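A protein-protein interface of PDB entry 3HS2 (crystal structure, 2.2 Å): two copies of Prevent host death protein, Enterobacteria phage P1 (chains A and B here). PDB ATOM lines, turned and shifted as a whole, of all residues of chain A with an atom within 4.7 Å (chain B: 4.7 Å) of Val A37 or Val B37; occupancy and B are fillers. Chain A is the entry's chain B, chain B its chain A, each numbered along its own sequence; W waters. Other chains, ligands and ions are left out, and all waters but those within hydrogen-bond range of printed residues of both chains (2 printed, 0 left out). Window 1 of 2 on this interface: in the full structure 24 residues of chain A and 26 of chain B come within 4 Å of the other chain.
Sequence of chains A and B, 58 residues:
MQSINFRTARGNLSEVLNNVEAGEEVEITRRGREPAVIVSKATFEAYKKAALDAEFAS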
ATOM      1  N   MET A   1       6.837  -0.597 -29.831  1.00  0.00           N
ATOM      2  CA  MET A   1       6.671  -0.766 -28.392  1.00  0.00           C
ATOM      3  C   MET A   1       5.952   0.431 -27.779  1.00  0.00           C
ATOM      4  O   MET A   1       6.401   1.571 -27.909  1.00  0.00           O
ATOM      5  CB  MET A   1       8.030  -0.964 -27.719  1.00  0.00           C
ATOM      6  CG  MET A   1       7.982  -0.976 -26.199  1.00  0.00           C
ATOM      7  SD  MET A   1       9.623  -0.976 -25.453  1.00  0.00           S
ATOM      8  CE  MET A   1      10.375  -2.374 -26.283  1.00  0.00           C
ATOM      9  N   GLU A  25       5.449  -5.606 -26.332  1.00  0.00           N
ATOM     10  CA  GLU A  25       6.448  -5.207 -25.343  1.00  0.00           C
ATOM     11  C   GLU A  25       6.086  -3.824 -24.827  1.00  0.00           C
ATOM     12  O   GLU A  25       5.795  -2.926 -25.614  1.00  0.00           O
ATOM     13  CB  GLU A  25       7.842  -5.163 -25.967  1.00  0.00           C
ATOM     14  CG  GLU A  25       8.213  -6.405 -26.758  1.00  0.00           C
ATOM     15  N   VAL A  26       6.099  -3.637 -23.513  1.00  0.00           N
ATOM     16  CA  VAL A  26       5.670  -2.358 -22.961  1.00  0.00           C
ATOM     17  C   VAL A  26       6.732  -1.696 -22.100  1.00  0.00           C
ATOM     18  O   VAL A  26       7.251  -2.294 -21.158  1.00  0.00           O
ATOM     19  CB  VAL A  26       4.369  -2.493 -22.150  1.00  0.00           C
ATOM     20  CG1 VAL A  26       3.859  -1.123 -21.741  1.00  0.00           C
ATOM     21  CG2 VAL A  26       3.321  -3.223 -22.962  1.00  0.00           C
ATOM     22  N   GLU A  27       7.041  -0.448 -22.434  1.00  0.00           N
ATOM     23  CA  GLU A  27       8.037   0.314 -21.704  1.00  0.00           C
ATOM     24  C   GLU A  27       7.411   1.111 -20.576  1.00  0.00           C
ATOM     25  O   GLU A  27       6.408   1.795 -20.762  1.00  0.00           O
ATOM     26  CB  GLU A  27       8.786   1.262 -22.636  1.00  0.00           C
ATOM     27  CG  GLU A  27       9.757   2.176 -21.907  1.00  0.00           C
ATOM     28  CD  GLU A  27      10.575   3.032 -22.851  1.00  0.00           C
ATOM     29  OE1 GLU A  27      10.049   3.427 -23.912  1.00  0.00           O
ATOM     30  OE2 GLU A  27      11.748   3.313 -22.529  1.00  0.00           O
ATOM     31  N   PRO A  35      14.401   3.512 -17.669  1.00  0.00           N
ATOM     32  CA  PRO A  35      13.155   2.849 -18.073  1.00  0.00           C
ATOM     33  C   PRO A  35      13.239   1.327 -17.962  1.00  0.00           C
ATOM     34  O   PRO A  35      14.294   0.730 -18.188  1.00  0.00           O
ATOM     35  CB  PRO A  35      12.983   3.271 -19.532  1.00  0.00           C
ATOM     36  CG  PRO A  35      14.337   3.652 -19.993  1.00  0.00           C
ATOM     37  CD  PRO A  35      15.113   4.117 -18.806  1.00  0.00           C
ATOM     38  N   ALA A  36      12.121   0.711 -17.598  1.00  0.00           N
ATOM     39  CA  ALA A  36      12.027  -0.738 -17.562  1.00  0.00           C
ATOM     40  C   ALA A  36      11.172  -1.215 -18.726  1.00  0.00           C
ATOM     41  O   ALA A  36      10.488  -0.422 -19.370  1.00  0.00           O
ATOM     42  CB  ALA A  36      11.431  -1.197 -16.240  1.00  0.00           C
ATOM     43  N   VAL A  37      11.219  -2.512 -19.002  1.00  0.00           N
ATOM     44  CA  VAL A  37      10.369  -3.084 -20.029  1.00  0.00           C
ATOM     45  C   VAL A  37       9.699  -4.351 -19.509  1.00  0.00           C
ATOM     46  O   VAL A  37      10.285  -5.104 -18.734  1.00  0.00           O
ATOM     47  CB  VAL A  37      11.158  -3.393 -21.315  1.00  0.00           C
ATOM     48  CG1 VAL A  37      11.982  -4.648 -21.140  1.00  0.00           C
ATOM     49  CG2 VAL A  37      10.211  -3.548 -22.489  1.00  0.00           C
ATOM     50  N   ILE A  38       8.458  -4.572 -19.920  1.00  0.00           N
ATOM     51  CA  ILE A  38       7.766  -5.800 -19.557  1.00  0.00           C
ATOM     52  C   ILE A  38       7.363  -6.585 -20.798  1.00  0.00           C
ATOM     53  O   ILE A  38       6.725  -6.051 -21.706  1.00  0.00           O
ATOM     54  CB  ILE A  38       6.554  -5.529 -18.651  1.00  0.00           C
ATOM     55  CG1 ILE A  38       5.555  -6.678 -18.753  1.00  0.00           C
ATOM     56  CG2 ILE A  38       5.900  -4.207 -19.007  1.00  0.00           C
ATOM     57  CD1 ILE A  38       4.815  -6.919 -17.480  1.00  0.00           C
ATOM     58  N   VAL A  39       7.748  -7.856 -20.824  1.00  0.00           N
ATOM     59  CA  VAL A  39       7.602  -8.695 -22.006  1.00  0.00           C
ATOM     60  C   VAL A  39       7.240 -10.112 -21.580  1.00  0.00           C
ATOM     61  O   VAL A  39       7.548 -10.528 -20.460  1.00  0.00           O
ATOM     62  CB  VAL A  39       8.918  -8.709 -22.823  1.00  0.00           C
ATOM     63  CG1 VAL A  39      10.075  -9.181 -21.958  1.00  0.00           C
ATOM     64  CG2 VAL A  39       8.784  -9.577 -24.058  1.00  0.00           C
ATOM     65  N   SER A  40       6.576 -10.853 -22.462  1.00  0.00           N
ATOM     66  CA  SER A  40       6.194 -12.219 -22.135  1.00  0.00           C
ATOM     67  C   SER A  40       7.438 -12.988 -21.717  1.00  0.00           C
ATOM     68  O   SER A  40       8.535 -12.728 -22.212  1.00  0.00           O
ATOM     69  CB  SER A  40       5.499 -12.902 -23.316  1.00  0.00           C
ATOM     70  OG  SER A  40       6.435 -13.445 -24.229  1.00  0.00           O
ATOM     71  N   LYS A  41       7.262 -13.919 -20.789  1.00  0.00           N
ATOM     72  CA  LYS A  41       8.375 -14.684 -20.249  1.00  0.00           C
ATOM     73  C   LYS A  41       9.039 -15.527 -21.329  1.00  0.00           C
ATOM     74  O   LYS A  41      10.266 -15.597 -21.408  1.00  0.00           O
ATOM     75  CB  LYS A  41       7.893 -15.579 -19.111  1.00  0.00           C
ATOM     76  CG  LYS A  41       8.991 -16.376 -18.436  1.00  0.00           C
ATOM     77  CD  LYS A  41       8.431 -17.177 -17.278  1.00  0.00           C
ATOM     78  CE  LYS A  41       9.526 -17.609 -16.322  1.00  0.00           C
ATOM     79  NZ  LYS A  41      10.369 -18.693 -16.887  1.00  0.00           N
ATOM     80  N   PHE A  44      11.109 -13.330 -23.568  1.00  0.00           N
ATOM     81  CA  PHE A  44      12.323 -12.917 -22.870  1.00  0.00           C
ATOM     82  C   PHE A  44      13.372 -14.021 -22.835  1.00  0.00           C
ATOM     83  O   PHE A  44      14.552 -13.777 -23.089  1.00  0.00           O
ATOM     84  CB  PHE A  44      12.008 -12.468 -21.443  1.00  0.00           C
ATOM     85  CG  PHE A  44      13.214 -11.991 -20.684  1.00  0.00           C
ATOM     86  CD1 PHE A  44      13.850 -10.817 -21.046  1.00  0.00           C
ATOM     87  CD2 PHE A  44      13.714 -12.717 -19.615  1.00  0.00           C
ATOM     88  CE1 PHE A  44      14.959 -10.373 -20.358  1.00  0.00           C
ATOM     89  CE2 PHE A  44      14.823 -12.276 -18.922  1.00  0.00           C
ATOM     90  CZ  PHE A  44      15.446 -11.101 -19.295  1.00  0.00           C
ATOM     91  N   MET B   1      15.481 -16.847 -11.221  1.00  0.00           N
ATOM     92  CA  MET B   1      14.897 -15.516 -11.344  1.00  0.00           C
ATOM     93  C   MET B   1      13.892 -15.268 -10.225  1.00  0.00           C
ATOM     94  O   MET B   1      13.216 -16.190  -9.771  1.00  0.00           O
ATOM     95  CB  MET B   1      14.223 -15.357 -12.711  1.00  0.00           C
ATOM     96  CG  MET B   1      13.632 -13.979 -12.974  1.00  0.00           C
ATOM     97  SD  MET B   1      13.140 -13.735 -14.695  1.00  0.00           S
ATOM     98  CE  MET B   1      12.162 -15.208 -14.979  1.00  0.00           C
ATOM     99  N   VAL B  26      12.661  -9.800 -12.921  1.00  0.00           N
ATOM    100  CA  VAL B  26      11.524 -10.150 -12.079  1.00  0.00           C
ATOM    101  C   VAL B  26      10.380 -10.756 -12.870  1.00  0.00           C
ATOM    102  O   VAL B  26       9.854 -10.147 -13.800  1.00  0.00           O
ATOM    103  CB  VAL B  26      11.016  -8.937 -11.282  1.00  0.00           C
ATOM    104  CG1 VAL B  26       9.695  -9.257 -10.605  1.00  0.00           C
ATOM    105  CG2 VAL B  26      12.054  -8.520 -10.260  1.00  0.00           C
ATOM    106  N   GLU B  27      10.003 -11.969 -12.487  1.00  0.00           N
ATOM    107  CA  GLU B  27       8.896 -12.661 -13.116  1.00  0.00           C
ATOM    108  C   GLU B  27       7.599 -12.323 -12.402  1.00  0.00           C
ATOM    109  O   GLU B  27       7.513 -12.379 -11.176  1.00  0.00           O
ATOM    110  CB  GLU B  27       9.135 -14.172 -13.092  1.00  0.00           C
ATOM    111  CG  GLU B  27       8.008 -15.003 -13.686  1.00  0.00           C
ATOM    112  CD  GLU B  27       8.225 -16.492 -13.494  1.00  0.00           C
ATOM    113  OE1 GLU B  27       9.306 -16.876 -13.001  1.00  0.00           O
ATOM    114  OE2 GLU B  27       7.318 -17.281 -13.834  1.00  0.00           O
ATOM    115  N   PRO B  35       3.123 -16.115 -17.666  1.00  0.00           N
ATOM    116  CA  PRO B  35       3.950 -15.202 -16.873  1.00  0.00           C
ATOM    117  C   PRO B  35       4.585 -14.111 -17.725  1.00  0.00           C
ATOM    118  O   PRO B  35       4.847 -14.304 -18.914  1.00  0.00           O
ATOM    119  CB  PRO B  35       5.038 -16.120 -16.296  1.00  0.00           C
ATOM    120  CG  PRO B  35       4.578 -17.522 -16.568  1.00  0.00           C
ATOM    121  CD  PRO B  35       3.743 -17.437 -17.800  1.00  0.00           C
ATOM    122  N   ALA B  36       4.819 -12.962 -17.103  1.00  0.00           N
ATOM    123  CA  ALA B  36       5.517 -11.866 -17.748  1.00  0.00           C
ATOM    124  C   ALA B  36       6.841 -11.634 -17.037  1.00  0.00           C
ATOM    125  O   ALA B  36       7.027 -12.059 -15.896  1.00  0.00           O
ATOM    126  CB  ALA B  36       4.669 -10.603 -17.711  1.00  0.00           C
ATOM    127  N   VAL B  37       7.767 -10.972 -17.720  1.00  0.00           N
ATOM    128  CA  VAL B  37       9.037 -10.607 -17.115  1.00  0.00           C
ATOM    129  C   VAL B  37       9.232  -9.100 -17.221  1.00  0.00           C
ATOM    130  O   VAL B  37       8.959  -8.503 -18.260  1.00  0.00           O
ATOM    131  CB  VAL B  37      10.225 -11.328 -17.783  1.00  0.00           C
ATOM    132  CG1 VAL B  37      11.540 -10.808 -17.228  1.00  0.00           C
ATOM    133  CG2 VAL B  37      10.123 -12.831 -17.578  1.00  0.00           C
ATOM    134  N   ILE B  38       9.683  -8.487 -16.135  1.00  0.00           N
ATOM    135  CA  ILE B  38      10.026  -7.073 -16.151  1.00  0.00           C
ATOM    136  C   ILE B  38      11.528  -6.916 -15.964  1.00  0.00           C
ATOM    137  O   ILE B  38      12.097  -7.408 -14.992  1.00  0.00           O
ATOM    138  CB  ILE B  38       9.263  -6.288 -15.071  1.00  0.00           C
ATOM    139  CG1 ILE B  38       9.764  -4.847 -14.999  1.00  0.00           C
ATOM    140  CG2 ILE B  38       9.400  -6.961 -13.717  1.00  0.00           C
ATOM    141  CD1 ILE B  38       8.851  -3.948 -14.210  1.00  0.00           C
ATOM    142  N   VAL B  39      12.165  -6.233 -16.910  1.00  0.00           N
ATOM    143  CA  VAL B  39      13.617  -6.116 -16.933  1.00  0.00           C
ATOM    144  C   VAL B  39      14.001  -4.733 -17.444  1.00  0.00           C
ATOM    145  O   VAL B  39      13.218  -4.084 -18.140  1.00  0.00           O
ATOM    146  CB  VAL B  39      14.235  -7.215 -17.834  1.00  0.00           C
ATOM    147  CG1 VAL B  39      13.676  -7.127 -19.243  1.00  0.00           C
ATOM    148  CG2 VAL B  39      15.752  -7.129 -17.845  1.00  0.00           C
ATOM    149  N   SER B  40      15.196  -4.271 -17.092  1.00  0.00           N
ATOM    150  CA  SER B  40      15.639  -2.958 -17.538  1.00  0.00           C
ATOM    151  C   SER B  40      15.612  -2.906 -19.059  1.00  0.00           C
ATOM    152  O   SER B  40      16.012  -3.859 -19.730  1.00  0.00           O
ATOM    153  CB  SER B  40      17.045  -2.643 -17.032  1.00  0.00           C
ATOM    154  OG  SER B  40      18.016  -2.894 -18.032  1.00  0.00           O
ATOM    155  N   LYS B  41      15.128  -1.792 -19.595  1.00  0.00           N
ATOM    156  CA  LYS B  41      15.016  -1.627 -21.033  1.00  0.00           C
ATOM    157  C   LYS B  41      16.377  -1.759 -21.711  1.00  0.00           C
ATOM    158  O   LYS B  41      16.488  -2.354 -22.782  1.00  0.00           O
ATOM    159  CB  LYS B  41      14.392  -0.272 -21.367  1.00  0.00           C
ATOM    160  CG  LYS B  41      14.200  -0.039 -22.853  1.00  0.00           C
ATOM    161  CD  LYS B  41      14.028   1.438 -23.153  1.00  0.00           C
ATOM    162  CE  LYS B  41      13.860   1.686 -24.643  1.00  0.00           C
ATOM    163  NZ  LYS B  41      13.746   3.136 -24.954  1.00  0.00           N
ATOM    164  N   PHE B  44      17.289  -5.423 -21.962  1.00  0.00           N
ATOM    165  CA  PHE B  44      16.444  -6.089 -22.950  1.00  0.00           C
ATOM    166  C   PHE B  44      16.841  -5.710 -24.374  1.00  0.00           C
ATOM    167  O   PHE B  44      16.895  -6.566 -25.260  1.00  0.00           O
ATOM    168  CB  PHE B  44      14.968  -5.770 -22.704  1.00  0.00           C
ATOM    169  CG  PHE B  44      14.026  -6.555 -23.573  1.00  0.00           C
ATOM    170  CD1 PHE B  44      14.055  -7.936 -23.567  1.00  0.00           C
ATOM    171  CD2 PHE B  44      13.104  -5.912 -24.382  1.00  0.00           C
ATOM    172  CE1 PHE B  44      13.194  -8.660 -24.358  1.00  0.00           C
ATOM    173  CE2 PHE B  44      12.238  -6.636 -25.173  1.00  0.00           C
ATOM    174  CZ  PHE B  44      12.285  -8.011 -25.160  1.00  0.00           C
HETATM  175  O   HOH W   1      17.272   0.884 -18.996  1.00  0.00           O
HETATM  176  O   HOH W   2       5.208 -16.439 -21.172  1.00  0.00           O
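Pro A35 touches Ser B40, but with the chains exchanged Ser A40 does not touch Pro B35 (4.04 Å).
Val A37 touches Ile B38, and with the chains exchanged Ile A38 touches Val B37.
Lys A41 touches Met B1, but with the chains exchanged Met A1 does not touch Lys B41 (5.1 Å).
Lys A41 touches Val B37, but with the chains exchanged Val A37 does not touch Lys B41 (4.02 Å).
11 positions are printed for both chains.
Of the 21 pairs that touch across the chains among the printed residues, 16 have their exchanged pair printed and touching as well.
Ala A36 touches Val B39 (C to O, 3.6 Å).
Val A37 touches Ile B38 (O to CA, 3.3 Å).
Val A37 touches Phe B44 (CG1 to CB, 3.6 Å).
Ile A38 touches Ala B36 (CD1 to CB, 3.7 Å).
CA of Ile A38 touches O of Val B37, at 3.2 Å.
Val A39 touches Ala B36 (O to CA, 3.6 Å).
Lys A41 touches Met B1.
CG2 of Val B37 touches CA of Lys A41, at 3.7 Å.
CG1 of Val B37 touches CD2 of Phe A44 (3.8 Å).
Val B39 touches Phe A44.
Water W1 bridges the backbone carbonyl oxygen (O) of Pro A35 (3.1 Å) and the backbone NH (N) of Lys B41 (3.5 Å).
Water W2 bridges O of Pro B35 and N of Lys A41.
N of Val B37 lies within hydrogen-bond range of O of Val A39, 2.8 Å away.
The backbone carbonyl oxygen of Val B39 lies within hydrogen-bond range of the backbone NH of Val A37 (2.7 Å).
The side-chain amino group (NZ) of Lys B41 is in salt-bridge range of the side-chain carboxylate (OE2) of Glu A27, at 3.1 Å.
The backbone carbonyl oxygen of Pro A35 is in hydrogen-bond range of the backbone NH of Lys B41 (3.0 Å).
The backbone carbonyl oxygen of Pro B35 sits at hydrogen-bond distance from the backbone NH of Lys A41 (3.1 Å).
Glu A25 touches none of the printed residues of chain B.
Val A26 touches none of the printed residues of chain B.
Printed residues of chain B within 4 Å of Pro A35: Ser B40 and Lys B41.
Of the printed residues of chain B, Val A37 touches Val B37, Ile B38, Val B39 and Phe B44.
Of the printed residues of chain A, Glu B27 touches Lys A41.
Val B37 touches just these residues of chain A: Val A37, Ile A38, Val A39, Lys A41 and Phe A44.
Of the 11 printed residues of chain B, 10 touch a printed residue of chain A.
Hydrophobic or aromatic side chains of chain B that line the printed part of chain A: Met B1, Pro B35, Ala B36, Val B37, Ile B38, Val B39 and Phe B44.
Of the 12 printed residues of chain A, 8 touch a printed residue of chain B.
Printed residues of chain A that touch a printed residue of chain B: Glu A27, Pro A35, Ala A36, Val A37, Ile A38, Val A39, Lys A41 and Phe A44.
Hydrophobic or aromatic side chains of chain A within 4 Å of the printed part of chain B: Pro A35, Ala A36, Val A37, Ile A38, Val A39 and Phe A44.
Among the printed residues, 21 pairs touch across the chains.
The backbone carbonyl oxygen of Val A26 is in hydrogen-bond range of the backbone NH of Ile A38, at 2.9 Å.
The backbone carbonyl oxygen of Val B26 sits at hydrogen-bond distance from the backbone NH of Ile B38, 2.9 Å away.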
